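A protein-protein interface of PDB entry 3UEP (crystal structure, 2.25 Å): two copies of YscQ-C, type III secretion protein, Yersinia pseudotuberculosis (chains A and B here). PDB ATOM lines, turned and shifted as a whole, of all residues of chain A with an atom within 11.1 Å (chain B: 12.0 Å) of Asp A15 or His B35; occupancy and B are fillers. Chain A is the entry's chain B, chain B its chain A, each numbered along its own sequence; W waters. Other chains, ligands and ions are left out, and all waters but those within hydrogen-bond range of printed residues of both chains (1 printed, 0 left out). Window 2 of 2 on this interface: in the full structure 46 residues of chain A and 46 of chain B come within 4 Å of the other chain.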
ATOM      1  N   PRO A  12      14.623   3.432   0.385  1.00  0.00           N
ATOM      2  CA  PRO A  12      14.461   2.064  -0.119  1.00  0.00           C
ATOM      3  C   PRO A  12      13.724   2.034  -1.454  1.00  0.00           C
ATOM      4  O   PRO A  12      12.739   2.751  -1.645  1.00  0.00           O
ATOM      5  CB  PRO A  12      13.633   1.374   0.974  1.00  0.00           C
ATOM      6  CG  PRO A  12      12.929   2.484   1.680  1.00  0.00           C
ATOM      7  CD  PRO A  12      13.875   3.652   1.637  1.00  0.00           C
ATOM      8  N   LEU A  13      14.217   1.196  -2.360  1.00  0.00           N
ATOM      9  CA  LEU A  13      13.681   1.077  -3.703  1.00  0.00           C
ATOM     10  C   LEU A  13      12.673  -0.055  -3.800  1.00  0.00           C
ATOM     11  O   LEU A  13      13.001  -1.204  -3.526  1.00  0.00           O
ATOM     12  CB  LEU A  13      14.821   0.794  -4.680  1.00  0.00           C
ATOM     13  CG  LEU A  13      15.948   1.822  -4.781  1.00  0.00           C
ATOM     14  CD1 LEU A  13      17.050   1.267  -5.641  1.00  0.00           C
ATOM     15  CD2 LEU A  13      15.425   3.136  -5.361  1.00  0.00           C
ATOM     16  N   THR A  14      11.454   0.273  -4.213  1.00  0.00           N
ATOM     17  CA  THR A  14      10.427  -0.728  -4.483  1.00  0.00           C
ATOM     18  C   THR A  14      10.905  -1.678  -5.580  1.00  0.00           C
ATOM     19  O   THR A  14      10.488  -2.839  -5.662  1.00  0.00           O
ATOM     20  CB  THR A  14       9.111  -0.061  -4.933  1.00  0.00           C
ATOM     21  OG1 THR A  14       8.558   0.692  -3.844  1.00  0.00           O
ATOM     22  CG2 THR A  14       8.098  -1.109  -5.392  1.00  0.00           C
ATOM     23  N   ASP A  15      11.788  -1.174  -6.427  1.00  0.00           N
ATOM     24  CA  ASP A  15      12.323  -1.953  -7.528  1.00  0.00           C
ATOM     25  C   ASP A  15      13.850  -1.854  -7.552  1.00  0.00           C
ATOM     26  O   ASP A  15      14.412  -0.819  -7.919  1.00  0.00           O
ATOM     27  CB  ASP A  15      11.723  -1.446  -8.840  1.00  0.00           C
ATOM     28  CG  ASP A  15      12.290  -2.147 -10.045  1.00  0.00           C
ATOM     29  OD1 ASP A  15      12.895  -3.230  -9.884  1.00  0.00           O
ATOM     30  OD2 ASP A  15      12.127  -1.615 -11.162  1.00  0.00           O
ATOM     31  N   LEU A  16      14.527  -2.928  -7.166  1.00  0.00           N
ATOM     32  CA  LEU A  16      15.984  -2.929  -7.196  1.00  0.00           C
ATOM     33  C   LEU A  16      16.555  -2.727  -8.609  1.00  0.00           C
ATOM     34  O   LEU A  16      17.716  -2.358  -8.757  1.00  0.00           O
ATOM     35  CB  LEU A  16      16.528  -4.233  -6.623  1.00  0.00           C
ATOM     36  CG  LEU A  16      16.912  -4.193  -5.153  1.00  0.00           C
ATOM     37  CD1 LEU A  16      17.570  -5.511  -4.748  1.00  0.00           C
ATOM     38  CD2 LEU A  16      17.826  -3.010  -4.896  1.00  0.00           C
ATOM     39  N   ASN A  17      15.780  -2.993  -9.654  1.00  0.00           N
ATOM     40  CA  ASN A  17      16.291  -2.694 -10.997  1.00  0.00           C
ATOM     41  C   ASN A  17      16.583  -1.180 -11.201  1.00  0.00           C
ATOM     42  O   ASN A  17      17.282  -0.798 -12.132  1.00  0.00           O
ATOM     43  CB  ASN A  17      15.361  -3.242 -12.084  1.00  0.00           C
ATOM     44  CG  ASN A  17      15.239  -4.764 -12.051  1.00  0.00           C
ATOM     45  OD1 ASN A  17      16.233  -5.469 -12.122  1.00  0.00           O
ATOM     46  ND2 ASN A  17      14.006  -5.271 -11.937  1.00  0.00           N
ATOM     47  N   GLN A  18      16.070  -0.323 -10.321  1.00  0.00           N
ATOM     48  CA  GLN A  18      16.418   1.099 -10.356  1.00  0.00           C
ATOM     49  C   GLN A  18      17.778   1.402  -9.724  1.00  0.00           C
ATOM     50  O   GLN A  18      18.138   2.565  -9.558  1.00  0.00           O
ATOM     51  CB  GLN A  18      15.380   1.910  -9.580  1.00  0.00           C
ATOM     52  CG  GLN A  18      13.949   1.707 -10.012  1.00  0.00           C
ATOM     53  CD  GLN A  18      13.604   2.531 -11.216  1.00  0.00           C
ATOM     54  OE1 GLN A  18      14.163   2.337 -12.294  1.00  0.00           O
ATOM     55  NE2 GLN A  18      12.686   3.468 -11.044  1.00  0.00           N
ATOM     56  N   LEU A  19      18.518   0.378  -9.329  1.00  0.00           N
ATOM     57  CA  LEU A  19      19.686   0.614  -8.482  1.00  0.00           C
ATOM     58  C   LEU A  19      20.798   1.236  -9.316  1.00  0.00           C
ATOM     59  O   LEU A  19      21.071   0.780 -10.424  1.00  0.00           O
ATOM     60  CB  LEU A  19      20.162  -0.691  -7.818  1.00  0.00           C
ATOM     61  CG  LEU A  19      21.236  -0.529  -6.748  1.00  0.00           C
ATOM     62  CD1 LEU A  19      20.610  -0.094  -5.429  1.00  0.00           C
ATOM     63  CD2 LEU A  19      22.011  -1.822  -6.576  1.00  0.00           C
ATOM     64  N   PRO A  20      21.438   2.286  -8.787  1.00  0.00           N
ATOM     65  CA  PRO A  20      22.479   2.981  -9.544  1.00  0.00           C
ATOM     66  C   PRO A  20      23.818   2.266  -9.465  1.00  0.00           C
ATOM     67  O   PRO A  20      24.313   2.018  -8.372  1.00  0.00           O
ATOM     68  CB  PRO A  20      22.569   4.344  -8.844  1.00  0.00           C
ATOM     69  CG  PRO A  20      22.154   4.065  -7.444  1.00  0.00           C
ATOM     70  CD  PRO A  20      21.117   2.977  -7.523  1.00  0.00           C
ATOM     71  N   VAL A  21      24.376   1.950 -10.631  1.00  0.00           N
ATOM     72  CA  VAL A  21      25.676   1.333 -10.772  1.00  0.00           C
ATOM     73  C   VAL A  21      26.707   2.355 -11.290  1.00  0.00           C
ATOM     74  O   VAL A  21      26.467   3.054 -12.282  1.00  0.00           O
ATOM     75  CB  VAL A  21      25.580   0.175 -11.771  1.00  0.00           C
ATOM     76  CG1 VAL A  21      26.942  -0.484 -11.997  1.00  0.00           C
ATOM     77  CG2 VAL A  21      24.552  -0.834 -11.292  1.00  0.00           C
ATOM     78  N   VAL A  23      29.553   3.330 -13.437  1.00  0.00           N
ATOM     79  CA  VAL A  23      30.152   2.829 -14.676  1.00  0.00           C
ATOM     80  C   VAL A  23      31.126   3.826 -15.339  1.00  0.00           C
ATOM     81  O   VAL A  23      30.739   4.954 -15.681  1.00  0.00           O
ATOM     82  CB  VAL A  23      29.081   2.491 -15.715  1.00  0.00           C
ATOM     83  CG1 VAL A  23      28.090   1.443 -15.161  1.00  0.00           C
ATOM     84  CG2 VAL A  23      28.362   3.764 -16.147  1.00  0.00           C
ATOM     85  N   LEU A  65      33.335  -4.605 -18.220  1.00  0.00           N
ATOM     86  CA  LEU A  65      31.982  -5.011 -18.632  1.00  0.00           C
ATOM     87  C   LEU A  65      31.869  -5.275 -20.141  1.00  0.00           C
ATOM     88  O   LEU A  65      31.061  -6.092 -20.598  1.00  0.00           O
ATOM     89  CB  LEU A  65      30.996  -3.897 -18.290  1.00  0.00           C
ATOM     90  CG  LEU A  65      29.684  -4.272 -17.621  1.00  0.00           C
ATOM     91  CD1 LEU A  65      29.937  -4.677 -16.180  1.00  0.00           C
ATOM     92  CD2 LEU A  65      28.750  -3.090 -17.669  1.00  0.00           C
ATOM     93  N   LEU A  84      30.323  -7.443 -25.154  1.00  0.00           N
ATOM     94  CA  LEU A  84      30.158  -7.464 -23.706  1.00  0.00           C
ATOM     95  C   LEU A  84      30.795  -8.726 -23.134  1.00  0.00           C
ATOM     96  O   LEU A  84      31.027  -9.697 -23.859  1.00  0.00           O
ATOM     97  CB  LEU A  84      28.686  -7.365 -23.326  1.00  0.00           C
ATOM     98  CG  LEU A  84      28.061  -6.045 -23.787  1.00  0.00           C
ATOM     99  CD1 LEU A  84      26.550  -6.186 -23.972  1.00  0.00           C
ATOM    100  CD2 LEU A  84      28.395  -4.893 -22.834  1.00  0.00           C
ATOM    101  N   ILE A  89      29.128  -8.116 -10.491  1.00  0.00           N
ATOM    102  CA  ILE A  89      29.002  -6.797  -9.891  1.00  0.00           C
ATOM    103  C   ILE A  89      28.518  -6.872  -8.435  1.00  0.00           C
ATOM    104  O   ILE A  89      27.593  -7.618  -8.109  1.00  0.00           O
ATOM    105  CB  ILE A  89      28.054  -5.930 -10.731  1.00  0.00           C
ATOM    106  CG1 ILE A  89      28.693  -5.642 -12.092  1.00  0.00           C
ATOM    107  CG2 ILE A  89      27.736  -4.633 -10.013  1.00  0.00           C
ATOM    108  CD1 ILE A  89      27.760  -4.983 -13.107  1.00  0.00           C
ATOM    109  N   LEU A  91      26.788  -5.108  -5.220  1.00  0.00           N
ATOM    110  CA  LEU A  91      25.844  -4.052  -4.937  1.00  0.00           C
ATOM    111  C   LEU A  91      25.541  -3.986  -3.441  1.00  0.00           C
ATOM    112  O   LEU A  91      25.323  -5.013  -2.802  1.00  0.00           O
ATOM    113  CB  LEU A  91      24.554  -4.282  -5.729  1.00  0.00           C
ATOM    114  CG  LEU A  91      24.672  -4.818  -7.160  1.00  0.00           C
ATOM    115  CD1 LEU A  91      23.408  -5.562  -7.519  1.00  0.00           C
ATOM    116  CD2 LEU A  91      24.941  -3.714  -8.178  1.00  0.00           C
ATOM    117  N   GLU A  92      25.544  -2.777  -2.889  1.00  0.00           N
ATOM    118  CA  GLU A  92      25.128  -2.567  -1.512  1.00  0.00           C
ATOM    119  C   GLU A  92      23.710  -1.989  -1.506  1.00  0.00           C
ATOM    120  O   GLU A  92      23.446  -0.943  -2.114  1.00  0.00           O
ATOM    121  CB  GLU A  92      26.107  -1.639  -0.787  1.00  0.00           C
ATOM    122  CG  GLU A  92      27.581  -1.980  -1.012  1.00  0.00           C
ATOM    123  CD  GLU A  92      27.958  -3.371  -0.528  1.00  0.00           C
ATOM    124  OE1 GLU A  92      27.887  -3.626   0.696  1.00  0.00           O
ATOM    125  OE2 GLU A  92      28.333  -4.209  -1.379  1.00  0.00           O
ATOM    126  N   VAL A  93      22.797  -2.676  -0.824  1.00  0.00           N
ATOM    127  CA  VAL A  93      21.389  -2.311  -0.889  1.00  0.00           C
ATOM    128  C   VAL A  93      20.803  -1.998   0.484  1.00  0.00           C
ATOM    129  O   VAL A  93      20.981  -2.752   1.439  1.00  0.00           O
ATOM    130  CB  VAL A  93      20.568  -3.431  -1.563  1.00  0.00           C
ATOM    131  CG1 VAL A  93      19.129  -3.032  -1.675  1.00  0.00           C
ATOM    132  CG2 VAL A  93      21.137  -3.731  -2.941  1.00  0.00           C
ATOM    133  N   LEU A  94      20.103  -0.875   0.580  1.00  0.00           N
ATOM    134  CA  LEU A  94      19.552  -0.445   1.851  1.00  0.00           C
ATOM    135  C   LEU A  94      18.198  -1.095   2.055  1.00  0.00           C
ATOM    136  O   LEU A  94      17.294  -0.939   1.226  1.00  0.00           O
ATOM    137  CB  LEU A  94      19.429   1.076   1.889  1.00  0.00           C
ATOM    138  CG  LEU A  94      19.042   1.699   3.234  1.00  0.00           C
ATOM    139  CD1 LEU A  94      19.404   0.791   4.406  1.00  0.00           C
ATOM    140  CD2 LEU A  94      19.706   3.057   3.388  1.00  0.00           C
ATOM    141  N   GLN A  96      14.743  -1.322   3.783  1.00  0.00           N
ATOM    142  CA  GLN A  96      13.874  -0.228   4.238  1.00  0.00           C
ATOM    143  C   GLN A  96      14.409   0.635   5.378  1.00  0.00           C
ATOM    144  O   GLN A  96      14.285   1.860   5.335  1.00  0.00           O
ATOM    145  CB  GLN A  96      12.481  -0.755   4.575  1.00  0.00           C
ATOM    146  CG  GLN A  96      12.487  -1.923   5.533  1.00  0.00           C
ATOM    147  CD  GLN A  96      11.219  -2.739   5.426  1.00  0.00           C
ATOM    148  OE1 GLN A  96      10.781  -3.088   4.324  1.00  0.00           O
ATOM    149  NE2 GLN A  96      10.612  -3.040   6.570  1.00  0.00           N
ATOM    150  N   ARG B  29      29.639  10.034 -17.962  1.00  0.00           N
ATOM    151  CA  ARG B  29      28.850   9.795 -16.758  1.00  0.00           C
ATOM    152  C   ARG B  29      29.412   8.640 -15.968  1.00  0.00           C
ATOM    153  O   ARG B  29      30.237   7.862 -16.457  1.00  0.00           O
ATOM    154  CB  ARG B  29      27.426   9.340 -17.127  1.00  0.00           C
ATOM    155  CG  ARG B  29      27.406   7.959 -17.814  1.00  0.00           C
ATOM    156  CD  ARG B  29      26.308   7.850 -18.846  1.00  0.00           C
ATOM    157  NE  ARG B  29      25.006   7.969 -18.210  1.00  0.00           N
ATOM    158  CZ  ARG B  29      23.855   8.061 -18.863  1.00  0.00           C
ATOM    159  NH1 ARG B  29      23.836   8.050 -20.193  1.00  0.00           N
ATOM    160  NH2 ARG B  29      22.721   8.165 -18.181  1.00  0.00           N
ATOM    161  N   ILE B  31      27.027   6.935 -13.797  1.00  0.00           N
ATOM    162  CA  ILE B  31      25.847   6.220 -13.290  1.00  0.00           C
ATOM    163  C   ILE B  31      24.889   5.689 -14.359  1.00  0.00           C
ATOM    164  O   ILE B  31      24.298   6.462 -15.110  1.00  0.00           O
ATOM    165  CB  ILE B  31      25.015   7.066 -12.281  1.00  0.00           C
ATOM    166  CG1 ILE B  31      25.863   7.503 -11.084  1.00  0.00           C
ATOM    167  CG2 ILE B  31      23.845   6.254 -11.770  1.00  0.00           C
ATOM    168  CD1 ILE B  31      26.209   6.359 -10.128  1.00  0.00           C
ATOM    169  N   LEU B  32      24.737   4.366 -14.412  1.00  0.00           N
ATOM    170  CA  LEU B  32      23.637   3.734 -15.144  1.00  0.00           C
ATOM    171  C   LEU B  32      22.857   2.854 -14.171  1.00  0.00           C
ATOM    172  O   LEU B  32      23.456   2.126 -13.372  1.00  0.00           O
ATOM    173  CB  LEU B  32      24.168   2.861 -16.287  1.00  0.00           C
ATOM    174  CG  LEU B  32      24.931   3.565 -17.416  1.00  0.00           C
ATOM    175  CD1 LEU B  32      25.405   2.575 -18.456  1.00  0.00           C
ATOM    176  CD2 LEU B  32      24.071   4.613 -18.054  1.00  0.00           C
ATOM    177  N   ASP B  33      21.531   2.900 -14.215  1.00  0.00           N
ATOM    178  CA  ASP B  33      20.778   1.942 -13.413  1.00  0.00           C
ATOM    179  C   ASP B  33      20.858   0.530 -13.994  1.00  0.00           C
ATOM    180  O   ASP B  33      21.400   0.325 -15.072  1.00  0.00           O
ATOM    181  CB  ASP B  33      19.326   2.392 -13.171  1.00  0.00           C
ATOM    182  CG  ASP B  33      18.464   2.352 -14.423  1.00  0.00           C
ATOM    183  OD1 ASP B  33      17.317   2.833 -14.346  1.00  0.00           O
ATOM    184  OD2 ASP B  33      18.911   1.844 -15.473  1.00  0.00           O
ATOM    185  N   TRP B  34      20.323  -0.446 -13.271  1.00  0.00           N
ATOM    186  CA  TRP B  34      20.412  -1.839 -13.702  1.00  0.00           C
ATOM    187  C   TRP B  34      19.582  -2.138 -14.939  1.00  0.00           C
ATOM    188  O   TRP B  34      20.019  -2.900 -15.802  1.00  0.00           O
ATOM    189  CB  TRP B  34      20.026  -2.808 -12.576  1.00  0.00           C
ATOM    190  CG  TRP B  34      20.092  -4.239 -13.025  1.00  0.00           C
ATOM    191  CD1 TRP B  34      19.048  -5.031 -13.380  1.00  0.00           C
ATOM    192  CD2 TRP B  34      21.279  -5.028 -13.199  1.00  0.00           C
ATOM    193  NE1 TRP B  34      19.505  -6.271 -13.763  1.00  0.00           N
ATOM    194  CE2 TRP B  34      20.874  -6.290 -13.665  1.00  0.00           C
ATOM    195  CE3 TRP B  34      22.647  -4.781 -13.022  1.00  0.00           C
ATOM    196  CZ2 TRP B  34      21.784  -7.319 -13.930  1.00  0.00           C
ATOM    197  CZ3 TRP B  34      23.550  -5.804 -13.290  1.00  0.00           C
ATOM    198  CH2 TRP B  34      23.114  -7.055 -13.732  1.00  0.00           C
ATOM    199  N   HIS B  35      18.381  -1.571 -15.025  1.00  0.00           N
ATOM    200  CA  HIS B  35      17.581  -1.710 -16.258  1.00  0.00           C
ATOM    201  C   HIS B  35      18.453  -1.377 -17.471  1.00  0.00           C
ATOM    202  O   HIS B  35      18.460  -2.091 -18.466  1.00  0.00           O
ATOM    203  CB  HIS B  35      16.399  -0.743 -16.281  1.00  0.00           C
ATOM    204  CG  HIS B  35      15.220  -1.181 -15.469  1.00  0.00           C
ATOM    205  ND1 HIS B  35      14.534  -2.349 -15.716  1.00  0.00           N
ATOM    206  CD2 HIS B  35      14.581  -0.578 -14.438  1.00  0.00           C
ATOM    207  CE1 HIS B  35      13.526  -2.456 -14.863  1.00  0.00           C
ATOM    208  NE2 HIS B  35      13.535  -1.395 -14.082  1.00  0.00           N
ATOM    209  N   THR B  36      19.179  -0.270 -17.376  1.00  0.00           N
ATOM    210  CA  THR B  36      20.024   0.202 -18.470  1.00  0.00           C
ATOM    211  C   THR B  36      21.190  -0.751 -18.757  1.00  0.00           C
ATOM    212  O   THR B  36      21.433  -1.078 -19.913  1.00  0.00           O
ATOM    213  CB  THR B  36      20.533   1.649 -18.230  1.00  0.00           C
ATOM    214  OG1 THR B  36      19.419   2.507 -17.993  1.00  0.00           O
ATOM    215  CG2 THR B  36      21.257   2.172 -19.457  1.00  0.00           C
ATOM    216  N   LEU B  37      21.875  -1.229 -17.719  1.00  0.00           N
ATOM    217  CA  LEU B  37      23.002  -2.157 -17.921  1.00  0.00           C
ATOM    218  C   LEU B  37      22.558  -3.491 -18.469  1.00  0.00           C
ATOM    219  O   LEU B  37      23.214  -4.062 -19.344  1.00  0.00           O
ATOM    220  CB  LEU B  37      23.772  -2.428 -16.618  1.00  0.00           C
ATOM    221  CG  LEU B  37      24.812  -1.477 -16.029  1.00  0.00           C
ATOM    222  CD1 LEU B  37      25.417  -2.136 -14.813  1.00  0.00           C
ATOM    223  CD2 LEU B  37      25.896  -1.169 -17.018  1.00  0.00           C
ATOM    224  N   THR B  38      21.457  -4.015 -17.939  1.00  0.00           N
ATOM    225  CA  THR B  38      20.976  -5.320 -18.401  1.00  0.00           C
ATOM    226  C   THR B  38      20.408  -5.262 -19.813  1.00  0.00           C
ATOM    227  O   THR B  38      20.364  -6.270 -20.501  1.00  0.00           O
ATOM    228  CB  THR B  38      19.917  -5.933 -17.472  1.00  0.00           C
ATOM    229  OG1 THR B  38      19.732  -7.302 -17.838  1.00  0.00           O
ATOM    230  CG2 THR B  38      18.599  -5.213 -17.617  1.00  0.00           C
ATOM    231  N   SER B  39      19.975  -4.091 -20.257  1.00  0.00           N
ATOM    232  CA  SER B  39      19.490  -3.957 -21.645  1.00  0.00           C
ATOM    233  C   SER B  39      20.625  -3.774 -22.659  1.00  0.00           C
ATOM    234  O   SER B  39      20.402  -3.841 -23.857  1.00  0.00           O
ATOM    235  CB  SER B  39      18.529  -2.782 -21.763  1.00  0.00           C
ATOM    236  OG  SER B  39      19.261  -1.600 -21.500  1.00  0.00           O
ATOM    237  N   LEU B  40      21.844  -3.542 -22.188  1.00  0.00           N
ATOM    238  CA  LEU B  40      22.957  -3.316 -23.111  1.00  0.00           C
ATOM    239  C   LEU B  40      23.224  -4.536 -23.986  1.00  0.00           C
ATOM    240  O   LEU B  40      23.154  -5.672 -23.518  1.00  0.00           O
ATOM    241  CB  LEU B  40      24.218  -2.922 -22.353  1.00  0.00           C
ATOM    242  CG  LEU B  40      24.162  -1.540 -21.692  1.00  0.00           C
ATOM    243  CD1 LEU B  40      25.514  -1.228 -21.072  1.00  0.00           C
ATOM    244  CD2 LEU B  40      23.778  -0.474 -22.719  1.00  0.00           C
ATOM    245  N   GLU B  41      23.486  -4.289 -25.270  1.00  0.00           N
ATOM    246  CA  GLU B  41      23.920  -5.332 -26.190  1.00  0.00           C
ATOM    247  C   GLU B  41      24.744  -4.677 -27.307  1.00  0.00           C
ATOM    248  O   GLU B  41      24.758  -3.452 -27.431  1.00  0.00           O
ATOM    249  CB  GLU B  41      22.718  -6.088 -26.751  1.00  0.00           C
ATOM    250  CG  GLU B  41      21.782  -5.246 -27.587  1.00  0.00           C
ATOM    251  CD  GLU B  41      20.521  -6.008 -27.974  1.00  0.00           C
ATOM    252  OE1 GLU B  41      20.256  -7.065 -27.362  1.00  0.00           O
ATOM    253  OE2 GLU B  41      19.797  -5.554 -28.889  1.00  0.00           O
ATOM    254  N   SER B  44      24.186  -1.108 -28.964  1.00  0.00           N
ATOM    255  CA  SER B  44      23.602  -0.130 -28.032  1.00  0.00           C
ATOM    256  C   SER B  44      24.399   1.160 -28.048  1.00  0.00           C
ATOM    257  O   SER B  44      25.621   1.125 -28.120  1.00  0.00           O
ATOM    258  CB  SER B  44      23.565  -0.657 -26.598  1.00  0.00           C
ATOM    259  OG  SER B  44      22.708  -1.781 -26.470  1.00  0.00           O
ATOM    260  N   LEU B  45      23.707   2.297 -27.976  1.00  0.00           N
ATOM    261  CA  LEU B  45      24.377   3.599 -27.913  1.00  0.00           C
ATOM    262  C   LEU B  45      24.178   4.224 -26.551  1.00  0.00           C
ATOM    263  O   LEU B  45      23.088   4.159 -25.974  1.00  0.00           O
ATOM    264  CB  LEU B  45      23.832   4.550 -28.972  1.00  0.00           C
ATOM    265  CG  LEU B  45      23.959   4.066 -30.407  1.00  0.00           C
ATOM    266  CD1 LEU B  45      22.965   4.757 -31.356  1.00  0.00           C
ATOM    267  CD2 LEU B  45      25.385   4.269 -30.842  1.00  0.00           C
ATOM    268  N   ILE B  46      25.244   4.813 -26.024  1.00  0.00           N
ATOM    269  CA  ILE B  46      25.171   5.458 -24.735  1.00  0.00           C
ATOM    270  C   ILE B  46      25.639   6.879 -24.894  1.00  0.00           C
ATOM    271  O   ILE B  46      26.718   7.140 -25.436  1.00  0.00           O
ATOM    272  CB  ILE B  46      26.062   4.795 -23.681  1.00  0.00           C
ATOM    273  CG1 ILE B  46      25.661   3.341 -23.479  1.00  0.00           C
ATOM    274  CG2 ILE B  46      25.968   5.547 -22.349  1.00  0.00           C
ATOM    275  CD1 ILE B  46      26.601   2.602 -22.475  1.00  0.00           C
HETATM  276  O   HOH W   1      17.659   4.809 -11.553  1.00  0.00           O
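The backbone NH (N) of Val A21 lies within hydrogen-bond range of the backbone carbonyl oxygen (O) of Leu B32 (2.9 Å).
A ring nitrogen (NE2) of His B35 lies within hydrogen-bond range of the side-chain carboxylate of Asp A15 (3.2 Å).
N of Trp B34 sits at hydrogen-bond distance from O of Leu A19.
The backbone carbonyl oxygen of Val A23 sits close to the backbone carbonyl oxygen of Arg B29.
The backbone carbonyl oxygen (O) of Asn A17 lies within hydrogen-bond range of the backbone NH (N) of His B35 (3.2 Å).
The backbone carbonyl oxygen (O) of Asn A17 lies within hydrogen-bond range of the backbone NH (N) of Trp B34 (3.3 Å).
The backbone carbonyl oxygen (O) of His B35 lies within hydrogen-bond range of the side-chain hydroxyl (OG) of Ser B39.
The side-chain carboxylate (OD1) of Asp A15 is in hydrogen-bond range of the backbone NH (N) of Asn A17.
The backbone NH (N) of His B35 lies close to the side-chain carboxylate (OD2) of Asp B33, 3.5 Å away.
The side-chain carboxylate (OD2) of Asp B33 sits at hydrogen-bond distance from the side-chain hydroxyl (OG1) of Thr B36, at 2.7 Å.
The side-chain hydroxyl of Ser B44 sits at hydrogen-bond distance from the backbone carbonyl oxygen of Glu B41.
Among the printed residues, pairs that only touch across the chains: Leu A19 with Asp B33, Val A21 with Ile B31, Leu A84 with Leu B40, Leu A65 with Leu B37, Leu A84 with Glu B41, Val A21 with Leu B37, Gln A18 with His B35, Val A23 with Leu B32, Pro A20 with Ile B31, Gln A18 with Asp B33, Val A23 with Leu B37, Pro A20 with Leu B32 and Asn A17 with Asp B33.
No residue of chain B comes within 4 Å of Thr A14.
Asp A15 touches just one residue of chain B: His B35 (3.2 Å).
Leu A16 touches none of the printed residues of chain B.
Gln A18 touches two residues of chain B.
Of chain B, only Asp B33 and Trp B34 come within 4 Å of Leu A19.
Of the printed residues of chain B, Val A23 touches Arg B29 (3.1 Å), Leu B32 (3.7 Å) and Leu B37 (3.9 Å).
Of the printed residues of chain B, Leu A65 touches Leu B37 (3.5 Å).
Of the printed residues of chain B, Leu A84 touches Leu B40 and Glu B41.
Of chain A, only Asp A15, Asn A17 and Gln A18 come within 4 Å of His B35.
No residue of chain A comes within 4 Å of Thr B38.
The nearest residue of chain B that does not touch Asp A15 is Trp B34 (7.3 Å).
Hydrophobic or aromatic side chains of chain A that line the printed part of chain B: Pro A20, Val A21, Val A23, Leu A65 and Leu A84.
Hydrophobic or aromatic side chains of chain B that line the printed part of chain A: Ile B31, Leu B32, Trp B34, His B35 and Leu B37.
Among the printed residues, no Asp or Glu carboxylate lies within 4 Å of a Lys or Arg side-chain nitrogen of the other chain.
No position is printed for both chains.
Of the 19 pairs that touch across the chains among the printed residues, none has its exchanged pair printed and touching as well.
Water W1 bridges the backbone carbonyl oxygen of Gln A18 (3.0 Å) and the side-chain carboxylate of Asp B33 (3.4 Å).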
